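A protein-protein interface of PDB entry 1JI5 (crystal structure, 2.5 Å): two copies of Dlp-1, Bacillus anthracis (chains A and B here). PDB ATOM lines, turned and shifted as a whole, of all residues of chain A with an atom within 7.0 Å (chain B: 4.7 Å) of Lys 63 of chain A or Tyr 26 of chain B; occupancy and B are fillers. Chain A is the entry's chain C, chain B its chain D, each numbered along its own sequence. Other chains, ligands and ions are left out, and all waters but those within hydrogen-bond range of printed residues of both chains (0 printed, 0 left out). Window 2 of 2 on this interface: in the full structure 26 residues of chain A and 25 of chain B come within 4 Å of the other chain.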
ATOM      1  N   ILE A   3       2.420 -37.137 -10.602  1.00  0.00           N
ATOM      2  CA  ILE A   3       1.625 -35.946 -10.304  1.00  0.00           C
ATOM      3  C   ILE A   3       2.526 -34.818  -9.811  1.00  0.00           C
ATOM      4  O   ILE A   3       2.269 -33.640 -10.060  1.00  0.00           O
ATOM      5  CB  ILE A   3       0.564 -36.258  -9.227  1.00  0.00           C
ATOM      6  CG1 ILE A   3      -0.440 -37.265  -9.780  1.00  0.00           C
ATOM      7  CG2 ILE A   3      -0.149 -34.993  -8.790  1.00  0.00           C
ATOM      8  CD1 ILE A   3      -1.410 -37.785  -8.754  1.00  0.00           C
ATOM      9  N   GLU A   4       3.600 -35.186  -9.125  1.00  0.00           N
ATOM     10  CA  GLU A   4       4.507 -34.185  -8.607  1.00  0.00           C
ATOM     11  C   GLU A   4       5.346 -33.570  -9.722  1.00  0.00           C
ATOM     12  O   GLU A   4       5.633 -32.369  -9.708  1.00  0.00           O
ATOM     13  CB  GLU A   4       5.379 -34.797  -7.497  1.00  0.00           C
ATOM     14  CG  GLU A   4       5.400 -33.935  -6.223  1.00  0.00           C
ATOM     15  CD  GLU A   4       4.163 -33.002  -6.112  1.00  0.00           C
ATOM     16  OE1 GLU A   4       3.008 -33.505  -6.152  1.00  0.00           O
ATOM     17  OE2 GLU A   4       4.352 -31.762  -5.991  1.00  0.00           O
ATOM     18  N   ASN A   7       2.910 -31.290 -11.476  1.00  0.00           N
ATOM     19  CA  ASN A   7       2.589 -30.107 -10.690  1.00  0.00           C
ATOM     20  C   ASN A   7       3.733 -29.112 -10.640  1.00  0.00           C
ATOM     21  O   ASN A   7       3.502 -27.909 -10.465  1.00  0.00           O
ATOM     22  CB  ASN A   7       2.147 -30.484  -9.274  1.00  0.00           C
ATOM     23  CG  ASN A   7       0.654 -30.724  -9.181  1.00  0.00           C
ATOM     24  OD1 ASN A   7      -0.142 -29.867  -9.560  1.00  0.00           O
ATOM     25  ND2 ASN A   7       0.266 -31.892  -8.673  1.00  0.00           N
ATOM     26  N   ALA A  54      -2.174 -29.584 -16.214  1.00  0.00           N
ATOM     27  CA  ALA A  54      -3.149 -29.619 -15.126  1.00  0.00           C
ATOM     28  C   ALA A  54      -4.226 -30.651 -15.427  1.00  0.00           C
ATOM     29  O   ALA A  54      -4.538 -31.530 -14.614  1.00  0.00           O
ATOM     30  CB  ALA A  54      -3.776 -28.263 -14.961  1.00  0.00           C
ATOM     31  N   ILE A  57      -2.828 -34.316 -15.122  1.00  0.00           N
ATOM     32  CA  ILE A  57      -2.792 -34.883 -13.788  1.00  0.00           C
ATOM     33  C   ILE A  57      -4.235 -35.059 -13.334  1.00  0.00           C
ATOM     34  O   ILE A  57      -4.576 -35.979 -12.591  1.00  0.00           O
ATOM     35  CB  ILE A  57      -2.037 -33.965 -12.802  1.00  0.00           C
ATOM     36  CG1 ILE A  57      -2.998 -33.022 -12.100  1.00  0.00           C
ATOM     37  CG2 ILE A  57      -1.007 -33.132 -13.543  1.00  0.00           C
ATOM     38  CD1 ILE A  57      -2.275 -32.110 -11.184  1.00  0.00           C
ATOM     39  N   LEU A  58      -5.086 -34.168 -13.812  1.00  0.00           N
ATOM     40  CA  LEU A  58      -6.490 -34.223 -13.475  1.00  0.00           C
ATOM     41  C   LEU A  58      -7.084 -35.498 -14.075  1.00  0.00           C
ATOM     42  O   LEU A  58      -8.004 -36.080 -13.509  1.00  0.00           O
ATOM     43  CB  LEU A  58      -7.182 -32.984 -14.033  1.00  0.00           C
ATOM     44  CG  LEU A  58      -8.384 -32.407 -13.293  1.00  0.00           C
ATOM     45  CD1 LEU A  58      -8.100 -32.300 -11.819  1.00  0.00           C
ATOM     46  CD2 LEU A  58      -8.681 -31.036 -13.845  1.00  0.00           C
ATOM     47  N   ILE A  60      -5.377 -38.268 -14.505  1.00  0.00           N
ATOM     48  CA  ILE A  60      -4.782 -39.431 -13.874  1.00  0.00           C
ATOM     49  C   ILE A  60      -5.073 -39.456 -12.374  1.00  0.00           C
ATOM     50  O   ILE A  60      -4.293 -40.005 -11.595  1.00  0.00           O
ATOM     51  CB  ILE A  60      -3.250 -39.483 -14.119  1.00  0.00           C
ATOM     52  CG1 ILE A  60      -2.558 -38.265 -13.508  1.00  0.00           C
ATOM     53  CG2 ILE A  60      -2.974 -39.533 -15.605  1.00  0.00           C
ATOM     54  CD1 ILE A  60      -1.041 -38.297 -13.631  1.00  0.00           C
ATOM     55  N   GLY A  61      -6.196 -38.851 -11.985  1.00  0.00           N
ATOM     56  CA  GLY A  61      -6.608 -38.824 -10.587  1.00  0.00           C
ATOM     57  C   GLY A  61      -5.866 -37.891  -9.640  1.00  0.00           C
ATOM     58  O   GLY A  61      -6.051 -37.943  -8.418  1.00  0.00           O
ATOM     59  N   GLY A  62      -5.027 -37.026 -10.190  1.00  0.00           N
ATOM     60  CA  GLY A  62      -4.287 -36.115  -9.343  1.00  0.00           C
ATOM     61  C   GLY A  62      -5.034 -34.830  -9.072  1.00  0.00           C
ATOM     62  O   GLY A  62      -6.119 -34.607  -9.619  1.00  0.00           O
ATOM     63  N   LYS A  63      -4.459 -33.996  -8.208  1.00  0.00           N
ATOM     64  CA  LYS A  63      -5.039 -32.700  -7.872  1.00  0.00           C
ATOM     65  C   LYS A  63      -4.009 -31.616  -8.186  1.00  0.00           C
ATOM     66  O   LYS A  63      -3.014 -31.465  -7.479  1.00  0.00           O
ATOM     67  CB  LYS A  63      -5.446 -32.649  -6.397  1.00  0.00           C
ATOM     68  CG  LYS A  63      -6.777 -33.333  -6.115  1.00  0.00           C
ATOM     69  CD  LYS A  63      -6.720 -34.832  -6.399  1.00  0.00           C
ATOM     70  CE  LYS A  63      -8.112 -35.413  -6.659  1.00  0.00           C
ATOM     71  NZ  LYS A  63      -9.123 -35.020  -5.624  1.00  0.00           N
ATOM     72  N   PRO A  64      -4.233 -30.858  -9.275  1.00  0.00           N
ATOM     73  CA  PRO A  64      -3.338 -29.784  -9.709  1.00  0.00           C
ATOM     74  C   PRO A  64      -3.219 -28.613  -8.763  1.00  0.00           C
ATOM     75  O   PRO A  64      -4.218 -28.105  -8.252  1.00  0.00           O
ATOM     76  CB  PRO A  64      -3.925 -29.377 -11.056  1.00  0.00           C
ATOM     77  CG  PRO A  64      -5.380 -29.641 -10.870  1.00  0.00           C
ATOM     78  CD  PRO A  64      -5.376 -30.981 -10.196  1.00  0.00           C
ATOM     79  N   VAL A  65      -1.982 -28.192  -8.526  1.00  0.00           N
ATOM     80  CA  VAL A  65      -1.730 -27.044  -7.666  1.00  0.00           C
ATOM     81  C   VAL A  65      -2.422 -25.874  -8.357  1.00  0.00           C
ATOM     82  O   VAL A  65      -2.323 -25.730  -9.577  1.00  0.00           O
ATOM     83  CB  VAL A  65      -0.212 -26.749  -7.536  1.00  0.00           C
ATOM     84  CG1 VAL A  65       0.451 -27.801  -6.653  1.00  0.00           C
ATOM     85  CG2 VAL A  65       0.438 -26.745  -8.913  1.00  0.00           C
ATOM     86  N   ALA A  66      -3.121 -25.041  -7.594  1.00  0.00           N
ATOM     87  CA  ALA A  66      -3.825 -23.943  -8.215  1.00  0.00           C
ATOM     88  C   ALA A  66      -3.882 -22.630  -7.439  1.00  0.00           C
ATOM     89  O   ALA A  66      -4.952 -22.043  -7.266  1.00  0.00           O
ATOM     90  CB  ALA A  66      -5.225 -24.398  -8.579  1.00  0.00           C
ATOM     91  N   ASN B  22      -8.314 -22.712 -11.466  1.00  0.00           N
ATOM     92  CA  ASN B  22      -8.609 -23.617 -10.363  1.00  0.00           C
ATOM     93  C   ASN B  22     -10.040 -24.093 -10.520  1.00  0.00           C
ATOM     94  O   ASN B  22     -10.294 -25.291 -10.603  1.00  0.00           O
ATOM     95  CB  ASN B  22      -8.451 -22.882  -9.028  1.00  0.00           C
ATOM     96  CG  ASN B  22      -8.673 -23.788  -7.819  1.00  0.00           C
ATOM     97  OD1 ASN B  22      -9.772 -24.308  -7.593  1.00  0.00           O
ATOM     98  ND2 ASN B  22      -7.624 -23.970  -7.029  1.00  0.00           N
ATOM     99  N   PHE B  23     -10.973 -23.146 -10.576  1.00  0.00           N
ATOM    100  CA  PHE B  23     -12.379 -23.492 -10.729  1.00  0.00           C
ATOM    101  C   PHE B  23     -12.591 -24.234 -12.038  1.00  0.00           C
ATOM    102  O   PHE B  23     -13.413 -25.146 -12.116  1.00  0.00           O
ATOM    103  CB  PHE B  23     -13.252 -22.235 -10.684  1.00  0.00           C
ATOM    104  CG  PHE B  23     -13.272 -21.552  -9.343  1.00  0.00           C
ATOM    105  CD1 PHE B  23     -12.450 -21.981  -8.310  1.00  0.00           C
ATOM    106  CD2 PHE B  23     -14.107 -20.464  -9.120  1.00  0.00           C
ATOM    107  CE1 PHE B  23     -12.457 -21.341  -7.081  1.00  0.00           C
ATOM    108  CE2 PHE B  23     -14.121 -19.816  -7.893  1.00  0.00           C
ATOM    109  CZ  PHE B  23     -13.294 -20.255  -6.873  1.00  0.00           C
ATOM    110  N   HIS B  24     -11.853 -23.842 -13.066  1.00  0.00           N
ATOM    111  CA  HIS B  24     -11.950 -24.501 -14.359  1.00  0.00           C
ATOM    112  C   HIS B  24     -11.599 -25.970 -14.148  1.00  0.00           C
ATOM    113  O   HIS B  24     -12.302 -26.847 -14.634  1.00  0.00           O
ATOM    114  CB  HIS B  24     -10.970 -23.848 -15.350  1.00  0.00           C
ATOM    115  CG  HIS B  24     -10.853 -24.550 -16.676  1.00  0.00           C
ATOM    116  ND1 HIS B  24     -11.925 -24.730 -17.526  1.00  0.00           N
ATOM    117  CD2 HIS B  24      -9.771 -25.046 -17.328  1.00  0.00           C
ATOM    118  CE1 HIS B  24     -11.508 -25.301 -18.643  1.00  0.00           C
ATOM    119  NE2 HIS B  24     -10.206 -25.503 -18.547  1.00  0.00           N
ATOM    120  N   TRP B  25     -10.529 -26.227 -13.390  1.00  0.00           N
ATOM    121  CA  TRP B  25     -10.061 -27.595 -13.130  1.00  0.00           C
ATOM    122  C   TRP B  25     -10.811 -28.422 -12.071  1.00  0.00           C
ATOM    123  O   TRP B  25     -11.032 -29.627 -12.247  1.00  0.00           O
ATOM    124  CB  TRP B  25      -8.577 -27.576 -12.751  1.00  0.00           C
ATOM    125  CG  TRP B  25      -7.672 -26.995 -13.799  1.00  0.00           C
ATOM    126  CD1 TRP B  25      -7.796 -27.121 -15.150  1.00  0.00           C
ATOM    127  CD2 TRP B  25      -6.477 -26.236 -13.575  1.00  0.00           C
ATOM    128  NE1 TRP B  25      -6.753 -26.489 -15.784  1.00  0.00           N
ATOM    129  CE2 TRP B  25      -5.929 -25.936 -14.839  1.00  0.00           C
ATOM    130  CE3 TRP B  25      -5.813 -25.783 -12.427  1.00  0.00           C
ATOM    131  CZ2 TRP B  25      -4.749 -25.201 -14.989  1.00  0.00           C
ATOM    132  CZ3 TRP B  25      -4.638 -25.052 -12.576  1.00  0.00           C
ATOM    133  CH2 TRP B  25      -4.122 -24.769 -13.849  1.00  0.00           C
ATOM    134  N   TYR B  26     -11.212 -27.785 -10.976  1.00  0.00           N
ATOM    135  CA  TYR B  26     -11.878 -28.502  -9.899  1.00  0.00           C
ATOM    136  C   TYR B  26     -13.414 -28.545  -9.883  1.00  0.00           C
ATOM    137  O   TYR B  26     -13.998 -29.255  -9.058  1.00  0.00           O
ATOM    138  CB  TYR B  26     -11.343 -27.974  -8.557  1.00  0.00           C
ATOM    139  CG  TYR B  26      -9.927 -28.429  -8.229  1.00  0.00           C
ATOM    140  CD1 TYR B  26      -9.662 -29.753  -7.872  1.00  0.00           C
ATOM    141  CD2 TYR B  26      -8.858 -27.541  -8.272  1.00  0.00           C
ATOM    142  CE1 TYR B  26      -8.364 -30.177  -7.558  1.00  0.00           C
ATOM    143  CE2 TYR B  26      -7.555 -27.957  -7.963  1.00  0.00           C
ATOM    144  CZ  TYR B  26      -7.317 -29.271  -7.603  1.00  0.00           C
ATOM    145  OH  TYR B  26      -6.042 -29.665  -7.261  1.00  0.00           O
ATOM    146  N   VAL B  27     -14.077 -27.818 -10.777  1.00  0.00           N
ATOM    147  CA  VAL B  27     -15.538 -27.838 -10.787  1.00  0.00           C
ATOM    148  C   VAL B  27     -16.097 -29.260 -11.018  1.00  0.00           C
ATOM    149  O   VAL B  27     -15.459 -30.091 -11.681  1.00  0.00           O
ATOM    150  CB  VAL B  27     -16.086 -26.884 -11.862  1.00  0.00           C
ATOM    151  CG1 VAL B  27     -15.709 -27.394 -13.245  1.00  0.00           C
ATOM    152  CG2 VAL B  27     -17.603 -26.737 -11.711  1.00  0.00           C
ATOM    153  N   LYS B  28     -17.282 -29.534 -10.459  1.00  0.00           N
ATOM    154  CA  LYS B  28     -17.933 -30.849 -10.584  1.00  0.00           C
ATOM    155  C   LYS B  28     -19.455 -30.742 -10.545  1.00  0.00           C
ATOM    156  O   LYS B  28     -20.004 -29.715 -10.143  1.00  0.00           O
ATOM    157  CB  LYS B  28     -17.471 -31.785  -9.463  1.00  0.00           C
ATOM    158  CG  LYS B  28     -15.971 -31.902  -9.373  1.00  0.00           C
ATOM    159  CD  LYS B  28     -15.511 -32.837  -8.281  1.00  0.00           C
ATOM    160  CE  LYS B  28     -13.971 -32.807  -8.191  1.00  0.00           C
ATOM    161  NZ  LYS B  28     -13.271 -33.061  -9.507  1.00  0.00           N
ATOM    162  N   TYR B  82      -9.967 -24.447  -2.338  1.00  0.00           N
ATOM    163  CA  TYR B  82     -10.257 -25.833  -2.696  1.00  0.00           C
ATOM    164  C   TYR B  82     -11.500 -26.289  -1.947  1.00  0.00           C
ATOM    165  O   TYR B  82     -11.958 -25.618  -1.018  1.00  0.00           O
ATOM    166  CB  TYR B  82      -9.094 -26.763  -2.339  1.00  0.00           C
ATOM    167  CG  TYR B  82      -7.783 -26.430  -3.010  1.00  0.00           C
ATOM    168  CD1 TYR B  82      -6.944 -25.443  -2.493  1.00  0.00           C
ATOM    169  CD2 TYR B  82      -7.380 -27.096  -4.168  1.00  0.00           C
ATOM    170  CE1 TYR B  82      -5.735 -25.126  -3.111  1.00  0.00           C
ATOM    171  CE2 TYR B  82      -6.175 -26.786  -4.796  1.00  0.00           C
ATOM    172  CZ  TYR B  82      -5.358 -25.796  -4.262  1.00  0.00           C
ATOM    173  OH  TYR B  82      -4.181 -25.452  -4.892  1.00  0.00           O
ATOM    174  N   MET B  89     -18.155 -21.795  -6.347  1.00  0.00           N
ATOM    175  CA  MET B  89     -17.257 -21.119  -7.274  1.00  0.00           C
ATOM    176  C   MET B  89     -17.952 -19.954  -7.989  1.00  0.00           C
ATOM    177  O   MET B  89     -17.410 -18.843  -8.058  1.00  0.00           O
ATOM    178  CB  MET B  89     -16.723 -22.128  -8.288  1.00  0.00           C
ATOM    179  CG  MET B  89     -15.898 -23.205  -7.642  1.00  0.00           C
ATOM    180  SD  MET B  89     -15.613 -24.620  -8.707  1.00  0.00           S
ATOM    181  CE  MET B  89     -14.127 -25.313  -7.964  1.00  0.00           C
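Among the printed residues, pairs that only touch across the chains: Lys 63 of chain A with Tyr 26 of chain B, Ala 54 of chain A with Trp 25 of chain B, Leu 58 of chain A with Trp 25 of chain B, Val 65 of chain A with Trp 25 of chain B and Val 65 of chain A with Tyr 82 of chain B.
OD1 of Asn 7 of chain A sits at hydrogen-bond distance from N of Val 65 of chain A (2.7 Å).
No position is printed for both chains.
Of the 13 printed residues of chain A, 6 touch a printed residue of chain B.
Along chain A the printed residues that touch a printed residue of chain B span positions 54 to 66.
Of the 9 printed residues of chain B, 4 touch a printed residue of chain A.
Among the printed residues, 8 pairs touch across the chains.
Among the printed residues, no Asp or Glu carboxylate lies within 4 Å of a Lys or Arg side-chain nitrogen of the other chain.
Lys 63 of chain A touches just one residue of chain B: Tyr 26.
Of chain A, only Lys 63 (3.0 Å) and Pro 64 (2.6 Å) come within 4 Å of Tyr 26 of chain B.
Printed residues of chain A within 4 Å of Tyr 82 of chain B: Val 65 (3.9 Å) and Ala 66 (2.9 Å).
Printed residues of chain A within 4 Å of Trp 25 of chain B: Ala 54 (3.2 Å), Leu 58 (3.2 Å) and Val 65 (3.8 Å).
Of the printed residues of chain A, Asn 22 of chain B touches Ala 66.
Of the printed residues of chain B, Leu 58 of chain A touches Trp 25 (3.2 Å).
Of the printed residues of chain B, Val 65 of chain A touches Trp 25 and Tyr 82.
The side-chain hydroxyl of Tyr 26 of chain B sits at hydrogen-bond distance from the backbone carbonyl oxygen of Pro 64 of chain A, 2.6 Å away.
ND2 of Asn 22 of chain B lies close to O of Ala 66 of chain A, at 3.3 Å.
N of Ala 66 of chain A is in hydrogen-bond range of OH of Tyr 82 of chain B (2.9 Å).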
